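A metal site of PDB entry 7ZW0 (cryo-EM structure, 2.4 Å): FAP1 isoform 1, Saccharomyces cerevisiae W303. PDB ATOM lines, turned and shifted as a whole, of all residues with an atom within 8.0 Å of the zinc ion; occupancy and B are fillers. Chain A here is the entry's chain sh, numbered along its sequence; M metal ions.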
ATOM      1  N   MET A  69     -10.234   7.224 -12.425  1.00  0.00           N
ATOM      2  CA  MET A  69      -9.015   6.413 -12.420  1.00  0.00           C
ATOM      3  C   MET A  69      -9.164   4.934 -12.748  1.00  0.00           C
ATOM      4  O   MET A  69      -8.357   4.390 -13.497  1.00  0.00           O
ATOM      5  CB  MET A  69      -8.285   6.580 -11.088  1.00  0.00           C
ATOM      6  CG  MET A  69      -7.801   7.996 -10.841  1.00  0.00           C
ATOM      7  SD  MET A  69      -6.785   8.172  -9.358  1.00  0.00           S
ATOM      8  CE  MET A  69      -5.390   7.133  -9.780  1.00  0.00           C
ATOM      9  N   PHE A  82     -16.839   9.983  -6.770  1.00  0.00           N
ATOM     10  CA  PHE A  82     -16.515   9.597  -5.388  1.00  0.00           C
ATOM     11  C   PHE A  82     -15.287  10.361  -4.887  1.00  0.00           C
ATOM     12  O   PHE A  82     -14.298  10.472  -5.615  1.00  0.00           O
ATOM     13  CB  PHE A  82     -16.250   8.110  -5.292  1.00  0.00           C
ATOM     14  CG  PHE A  82     -15.840   7.660  -3.916  1.00  0.00           C
ATOM     15  CD1 PHE A  82     -16.786   7.527  -2.918  1.00  0.00           C
ATOM     16  CD2 PHE A  82     -14.525   7.363  -3.631  1.00  0.00           C
ATOM     17  CE1 PHE A  82     -16.422   7.116  -1.644  1.00  0.00           C
ATOM     18  CE2 PHE A  82     -14.145   6.963  -2.368  1.00  0.00           C
ATOM     19  CZ  PHE A  82     -15.095   6.830  -1.379  1.00  0.00           C
ATOM     20  N   ALA A  83     -15.346  10.893  -3.677  1.00  0.00           N
ATOM     21  CA  ALA A  83     -14.240  11.688  -3.158  1.00  0.00           C
ATOM     22  C   ALA A  83     -13.603  11.068  -1.934  1.00  0.00           C
ATOM     23  O   ALA A  83     -14.298  10.585  -1.040  1.00  0.00           O
ATOM     24  CB  ALA A  83     -14.694  13.101  -2.871  1.00  0.00           C
ATOM     25  N   CYS A  84     -12.282  11.086  -1.876  1.00  0.00           N
ATOM     26  CA  CYS A  84     -11.583  10.573  -0.706  1.00  0.00           C
ATOM     27  C   CYS A  84     -10.831  11.720  -0.078  1.00  0.00           C
ATOM     28  O   CYS A  84     -10.154  12.458  -0.778  1.00  0.00           O
ATOM     29  CB  CYS A  84     -10.614   9.450  -1.080  1.00  0.00           C
ATOM     30  SG  CYS A  84      -9.539   8.921   0.266  1.00  0.00           S
ATOM     31  N   LYS A  85     -10.937  11.884   1.231  1.00  0.00           N
ATOM     32  CA  LYS A  85     -10.304  13.022   1.876  1.00  0.00           C
ATOM     33  C   LYS A  85      -8.796  12.989   1.735  1.00  0.00           C
ATOM     34  O   LYS A  85      -8.168  14.014   1.520  1.00  0.00           O
ATOM     35  CB  LYS A  85     -10.690  13.081   3.366  1.00  0.00           C
ATOM     36  CG  LYS A  85     -12.084  13.642   3.647  1.00  0.00           C
ATOM     37  CD  LYS A  85     -13.181  12.600   3.461  1.00  0.00           C
ATOM     38  CE  LYS A  85     -14.008  12.874   2.225  1.00  0.00           C
ATOM     39  NZ  LYS A  85     -14.853  11.705   1.858  1.00  0.00           N
ATOM     40  N   ARG A  86      -8.206  11.807   1.841  1.00  0.00           N
ATOM     41  CA  ARG A  86      -6.756  11.708   1.785  1.00  0.00           C
ATOM     42  C   ARG A  86      -6.184  12.161   0.436  1.00  0.00           C
ATOM     43  O   ARG A  86      -5.190  12.889   0.399  1.00  0.00           O
ATOM     44  CB  ARG A  86      -6.308  10.280   2.119  1.00  0.00           C
ATOM     45  CG  ARG A  86      -4.839  10.173   2.502  1.00  0.00           C
ATOM     46  CD  ARG A  86      -4.543  10.961   3.763  1.00  0.00           C
ATOM     47  NE  ARG A  86      -3.117  11.226   3.927  1.00  0.00           N
ATOM     48  CZ  ARG A  86      -2.504  12.325   3.494  1.00  0.00           C
ATOM     49  NH1 ARG A  86      -3.196  13.268   2.878  1.00  0.00           N
ATOM     50  NH2 ARG A  86      -1.198  12.480   3.678  1.00  0.00           N
ATOM     51  N   CYS A  87      -6.813  11.756  -0.659  1.00  0.00           N
ATOM     52  CA  CYS A  87      -6.323  12.152  -1.978  1.00  0.00           C
ATOM     53  C   CYS A  87      -7.066  13.313  -2.604  1.00  0.00           C
ATOM     54  O   CYS A  87      -6.600  13.861  -3.604  1.00  0.00           O
ATOM     55  CB  CYS A  87      -6.404  10.973  -2.939  1.00  0.00           C
ATOM     56  SG  CYS A  87      -8.092  10.534  -3.405  1.00  0.00           S
ATOM     57  N   TYR A  88      -8.182  13.717  -2.022  1.00  0.00           N
ATOM     58  CA  TYR A  88      -9.016  14.760  -2.621  1.00  0.00           C
ATOM     59  C   TYR A  88      -9.086  14.657  -4.140  1.00  0.00           C
ATOM     60  O   TYR A  88      -8.927  15.657  -4.850  1.00  0.00           O
ATOM     61  CB  TYR A  88      -8.602  16.156  -2.152  1.00  0.00           C
ATOM     62  CG  TYR A  88      -9.187  16.494  -0.804  1.00  0.00           C
ATOM     63  CD1 TYR A  88     -10.548  16.336  -0.572  1.00  0.00           C
ATOM     64  CD2 TYR A  88      -8.395  16.974   0.221  1.00  0.00           C
ATOM     65  CE1 TYR A  88     -11.097  16.639   0.659  1.00  0.00           C
ATOM     66  CE2 TYR A  88      -8.930  17.278   1.455  1.00  0.00           C
ATOM     67  CZ  TYR A  88     -10.287  17.100   1.673  1.00  0.00           C
ATOM     68  OH  TYR A  88     -10.828  17.404   2.899  1.00  0.00           O
ATOM     69  N   ARG A  89      -9.338  13.455  -4.647  1.00  0.00           N
ATOM     70  CA  ARG A  89      -9.434  13.237  -6.074  1.00  0.00           C
ATOM     71  C   ARG A  89     -10.761  12.541  -6.348  1.00  0.00           C
ATOM     72  O   ARG A  89     -11.312  11.888  -5.457  1.00  0.00           O
ATOM     73  CB  ARG A  89      -8.240  12.395  -6.540  1.00  0.00           C
ATOM     74  CG  ARG A  89      -8.398  11.628  -7.842  1.00  0.00           C
ATOM     75  CD  ARG A  89      -7.668  12.300  -8.990  1.00  0.00           C
ATOM     76  NE  ARG A  89      -7.934  11.635 -10.261  1.00  0.00           N
ATOM     77  CZ  ARG A  89      -7.359  11.964 -11.419  1.00  0.00           C
ATOM     78  NH1 ARG A  89      -6.470  12.945 -11.455  1.00  0.00           N
ATOM     79  NH2 ARG A  89      -7.677  11.312 -12.528  1.00  0.00           N
ATOM     80  N   VAL A  90     -11.294  12.667  -7.554  1.00  0.00           N
ATOM     81  CA  VAL A  90     -12.589  12.074  -7.875  1.00  0.00           C
ATOM     82  C   VAL A  90     -12.570  11.005  -8.961  1.00  0.00           C
ATOM     83  O   VAL A  90     -11.876  11.150  -9.977  1.00  0.00           O
ATOM     84  CB  VAL A  90     -13.622  13.166  -8.183  1.00  0.00           C
ATOM     85  CG1 VAL A  90     -14.691  12.694  -9.137  1.00  0.00           C
ATOM     86  CG2 VAL A  90     -14.234  13.663  -6.893  1.00  0.00           C
ATOM     87  N   PHE A  91     -13.282   9.903  -8.739  1.00  0.00           N
ATOM     88  CA  PHE A  91     -13.356   8.835  -9.730  1.00  0.00           C
ATOM     89  C   PHE A  91     -14.831   8.567  -9.933  1.00  0.00           C
ATOM     90  O   PHE A  91     -15.652   9.061  -9.174  1.00  0.00           O
ATOM     91  CB  PHE A  91     -12.679   7.571  -9.202  1.00  0.00           C
ATOM     92  CG  PHE A  91     -11.797   7.803  -8.015  1.00  0.00           C
ATOM     93  CD1 PHE A  91     -12.328   7.776  -6.727  1.00  0.00           C
ATOM     94  CD2 PHE A  91     -10.444   8.050  -8.173  1.00  0.00           C
ATOM     95  CE1 PHE A  91     -11.513   7.995  -5.628  1.00  0.00           C
ATOM     96  CE2 PHE A  91      -9.634   8.258  -7.082  1.00  0.00           C
ATOM     97  CZ  PHE A  91     -10.170   8.241  -5.802  1.00  0.00           C
ATOM     98  N   ILE A  96     -15.113   3.077  -8.870  1.00  0.00           N
ATOM     99  CA  ILE A  96     -14.326   2.940  -7.660  1.00  0.00           C
ATOM    100  C   ILE A  96     -14.912   1.863  -6.735  1.00  0.00           C
ATOM    101  O   ILE A  96     -14.166   1.221  -5.995  1.00  0.00           O
ATOM    102  CB  ILE A  96     -14.156   4.291  -6.927  1.00  0.00           C
ATOM    103  CG1 ILE A  96     -12.927   4.265  -6.014  1.00  0.00           C
ATOM    104  CG2 ILE A  96     -15.388   4.652  -6.104  1.00  0.00           C
ATOM    105  CD1 ILE A  96     -11.629   4.038  -6.752  1.00  0.00           C
ATOM    106  N   TRP A 112     -10.926  -1.835   1.582  1.00  0.00           N
ATOM    107  CA  TRP A 112     -10.846  -1.199   0.269  1.00  0.00           C
ATOM    108  C   TRP A 112      -9.703  -0.177   0.189  1.00  0.00           C
ATOM    109  O   TRP A 112      -9.373   0.448   1.183  1.00  0.00           O
ATOM    110  CB  TRP A 112     -12.187  -0.551  -0.080  1.00  0.00           C
ATOM    111  CG  TRP A 112     -12.238   0.926   0.103  1.00  0.00           C
ATOM    112  CD1 TRP A 112     -12.477   1.606   1.257  1.00  0.00           C
ATOM    113  CD2 TRP A 112     -12.053   1.925  -0.920  1.00  0.00           C
ATOM    114  NE1 TRP A 112     -12.455   2.957   1.016  1.00  0.00           N
ATOM    115  CE2 TRP A 112     -12.191   3.175  -0.309  1.00  0.00           C
ATOM    116  CE3 TRP A 112     -11.782   1.865  -2.290  1.00  0.00           C
ATOM    117  CZ2 TRP A 112     -12.068   4.363  -1.012  1.00  0.00           C
ATOM    118  CZ3 TRP A 112     -11.661   3.042  -2.979  1.00  0.00           C
ATOM    119  CH2 TRP A 112     -11.801   4.282  -2.355  1.00  0.00           C
ATOM    120  N   LYS A 113      -9.106   0.003  -0.992  1.00  0.00           N
ATOM    121  CA  LYS A 113      -7.948   0.916  -1.102  1.00  0.00           C
ATOM    122  C   LYS A 113      -8.181   2.053  -2.088  1.00  0.00           C
ATOM    123  O   LYS A 113      -8.726   1.834  -3.157  1.00  0.00           O
ATOM    124  CB  LYS A 113      -6.698   0.127  -1.510  1.00  0.00           C
ATOM    125  CG  LYS A 113      -5.405   0.925  -1.406  1.00  0.00           C
ATOM    126  CD  LYS A 113      -4.205   0.001  -1.352  1.00  0.00           C
ATOM    127  CE  LYS A 113      -2.978   0.756  -0.874  1.00  0.00           C
ATOM    128  NZ  LYS A 113      -1.823  -0.164  -0.648  1.00  0.00           N
ATOM    129  N   CYS A 114      -7.763   3.251  -1.733  1.00  0.00           N
ATOM    130  CA  CYS A 114      -7.896   4.373  -2.640  1.00  0.00           C
ATOM    131  C   CYS A 114      -6.606   4.558  -3.408  1.00  0.00           C
ATOM    132  O   CYS A 114      -5.566   4.804  -2.808  1.00  0.00           O
ATOM    133  CB  CYS A 114      -8.236   5.645  -1.876  1.00  0.00           C
ATOM    134  SG  CYS A 114      -8.477   7.074  -2.947  1.00  0.00           S
ATOM    135  N   PRO A 115      -6.653   4.462  -4.740  1.00  0.00           N
ATOM    136  CA  PRO A 115      -5.430   4.522  -5.556  1.00  0.00           C
ATOM    137  C   PRO A 115      -4.635   5.826  -5.565  1.00  0.00           C
ATOM    138  O   PRO A 115      -3.407   5.758  -5.515  1.00  0.00           O
ATOM    139  CB  PRO A 115      -5.938   4.263  -6.981  1.00  0.00           C
ATOM    140  CG  PRO A 115      -7.304   3.665  -6.818  1.00  0.00           C
ATOM    141  CD  PRO A 115      -7.856   4.268  -5.569  1.00  0.00           C
ATOM    142  N   ASN A 116      -5.291   6.972  -5.628  1.00  0.00           N
ATOM    143  CA  ASN A 116      -4.540   8.225  -5.750  1.00  0.00           C
ATOM    144  C   ASN A 116      -3.655   8.497  -4.553  1.00  0.00           C
ATOM    145  O   ASN A 116      -2.505   8.919  -4.705  1.00  0.00           O
ATOM    146  CB  ASN A 116      -5.483   9.403  -5.998  1.00  0.00           C
ATOM    147  CG  ASN A 116      -4.760  10.604  -6.599  1.00  0.00           C
ATOM    148  OD1 ASN A 116      -4.081  10.476  -7.621  1.00  0.00           O
ATOM    149  ND2 ASN A 116      -4.921  11.762  -5.981  1.00  0.00           N
ATOM    150  N   CYS A 117      -4.165   8.252  -3.356  1.00  0.00           N
ATOM    151  CA  CYS A 117      -3.354   8.419  -2.157  1.00  0.00           C
ATOM    152  C   CYS A 117      -2.720   7.105  -1.779  1.00  0.00           C
ATOM    153  O   CYS A 117      -2.001   7.037  -0.776  1.00  0.00           O
ATOM    154  CB  CYS A 117      -4.198   8.942  -1.004  1.00  0.00           C
ATOM    155  SG  CYS A 117      -5.799   8.136  -0.864  1.00  0.00           S
ATOM    156  N   TYR A 118      -2.990   6.057  -2.551  1.00  0.00           N
ATOM    157  CA  TYR A 118      -2.478   4.725  -2.236  1.00  0.00           C
ATOM    158  C   TYR A 118      -2.770   4.471  -0.774  1.00  0.00           C
ATOM    159  O   TYR A 118      -1.908   4.009  -0.030  1.00  0.00           O
ATOM    160  CB  TYR A 118      -0.973   4.625  -2.540  1.00  0.00           C
ATOM    161  CG  TYR A 118      -0.493   3.222  -2.785  1.00  0.00           C
ATOM    162  CD1 TYR A 118      -1.014   2.452  -3.820  1.00  0.00           C
ATOM    163  CD2 TYR A 118       0.496   2.658  -1.989  1.00  0.00           C
ATOM    164  CE1 TYR A 118      -0.576   1.166  -4.041  1.00  0.00           C
ATOM    165  CE2 TYR A 118       0.948   1.373  -2.206  1.00  0.00           C
ATOM    166  CZ  TYR A 118       0.410   0.632  -3.243  1.00  0.00           C
ATOM    167  OH  TYR A 118       0.857  -0.653  -3.470  1.00  0.00           O
ATOM    168  N   TYR A 119      -3.990   4.781  -0.349  1.00  0.00           N
ATOM    169  CA  TYR A 119      -4.337   4.644   1.062  1.00  0.00           C
ATOM    170  C   TYR A 119      -5.503   3.719   1.250  1.00  0.00           C
ATOM    171  O   TYR A 119      -6.543   3.885   0.615  1.00  0.00           O
ATOM    172  CB  TYR A 119      -4.590   6.037   1.661  1.00  0.00           C
ATOM    173  CG  TYR A 119      -5.786   6.187   2.585  1.00  0.00           C
ATOM    174  CD1 TYR A 119      -7.037   6.524   2.092  1.00  0.00           C
ATOM    175  CD2 TYR A 119      -5.645   6.048   3.958  1.00  0.00           C
ATOM    176  CE1 TYR A 119      -8.125   6.675   2.924  1.00  0.00           C
ATOM    177  CE2 TYR A 119      -6.728   6.199   4.799  1.00  0.00           C
ATOM    178  CZ  TYR A 119      -7.957   6.508   4.281  1.00  0.00           C
ATOM    179  OH  TYR A 119      -9.045   6.659   5.113  1.00  0.00           O
ATOM    180  N   VAL A 120      -5.336   2.711   2.096  1.00  0.00           N
ATOM    181  CA  VAL A 120      -6.436   1.799   2.371  1.00  0.00           C
ATOM    182  C   VAL A 120      -7.420   2.416   3.337  1.00  0.00           C
ATOM    183  O   VAL A 120      -7.034   3.138   4.246  1.00  0.00           O
ATOM    184  CB  VAL A 120      -5.915   0.482   2.964  1.00  0.00           C
ATOM    185  CG1 VAL A 120      -6.326  -0.694   2.083  1.00  0.00           C
ATOM    186  CG2 VAL A 120      -4.411   0.533   3.107  1.00  0.00           C
ATOM    187  N   SER A 121      -8.697   2.122   3.162  1.00  0.00           N
ATOM    188  CA  SER A 121      -9.720   2.607   4.086  1.00  0.00           C
ATOM    189  C   SER A 121     -10.576   1.421   4.462  1.00  0.00           C
ATOM    190  O   SER A 121     -10.501   0.377   3.802  1.00  0.00           O
ATOM    191  CB  SER A 121     -10.531   3.752   3.481  1.00  0.00           C
ATOM    192  OG  SER A 121     -11.453   4.284   4.422  1.00  0.00           O
HETATM  193 ZN    ZN M   1      -8.134   8.751  -1.823  1.00  0.00          ZN
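SG of Cys 84 sits close to N of Arg 86, at 3.5 Å.
The backbone NH (N) of Cys 114 sits at hydrogen-bond distance from the backbone carbonyl oxygen (O) of Tyr 119 (2.7 Å).
N of Arg 89 sits close to SG of Cys 87, at 3.4 Å.
Along chain A the residues within 4 Å of the zinc ion span positions 84 to 117.
The zinc ion is bound by the side-chain sulfur of Cys 114, the side-chain sulfur of Cys 87, the side-chain sulfur of Cys 84 and the side-chain sulfur of Cys 117.
The zinc ion has four donor atoms within binding distance.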
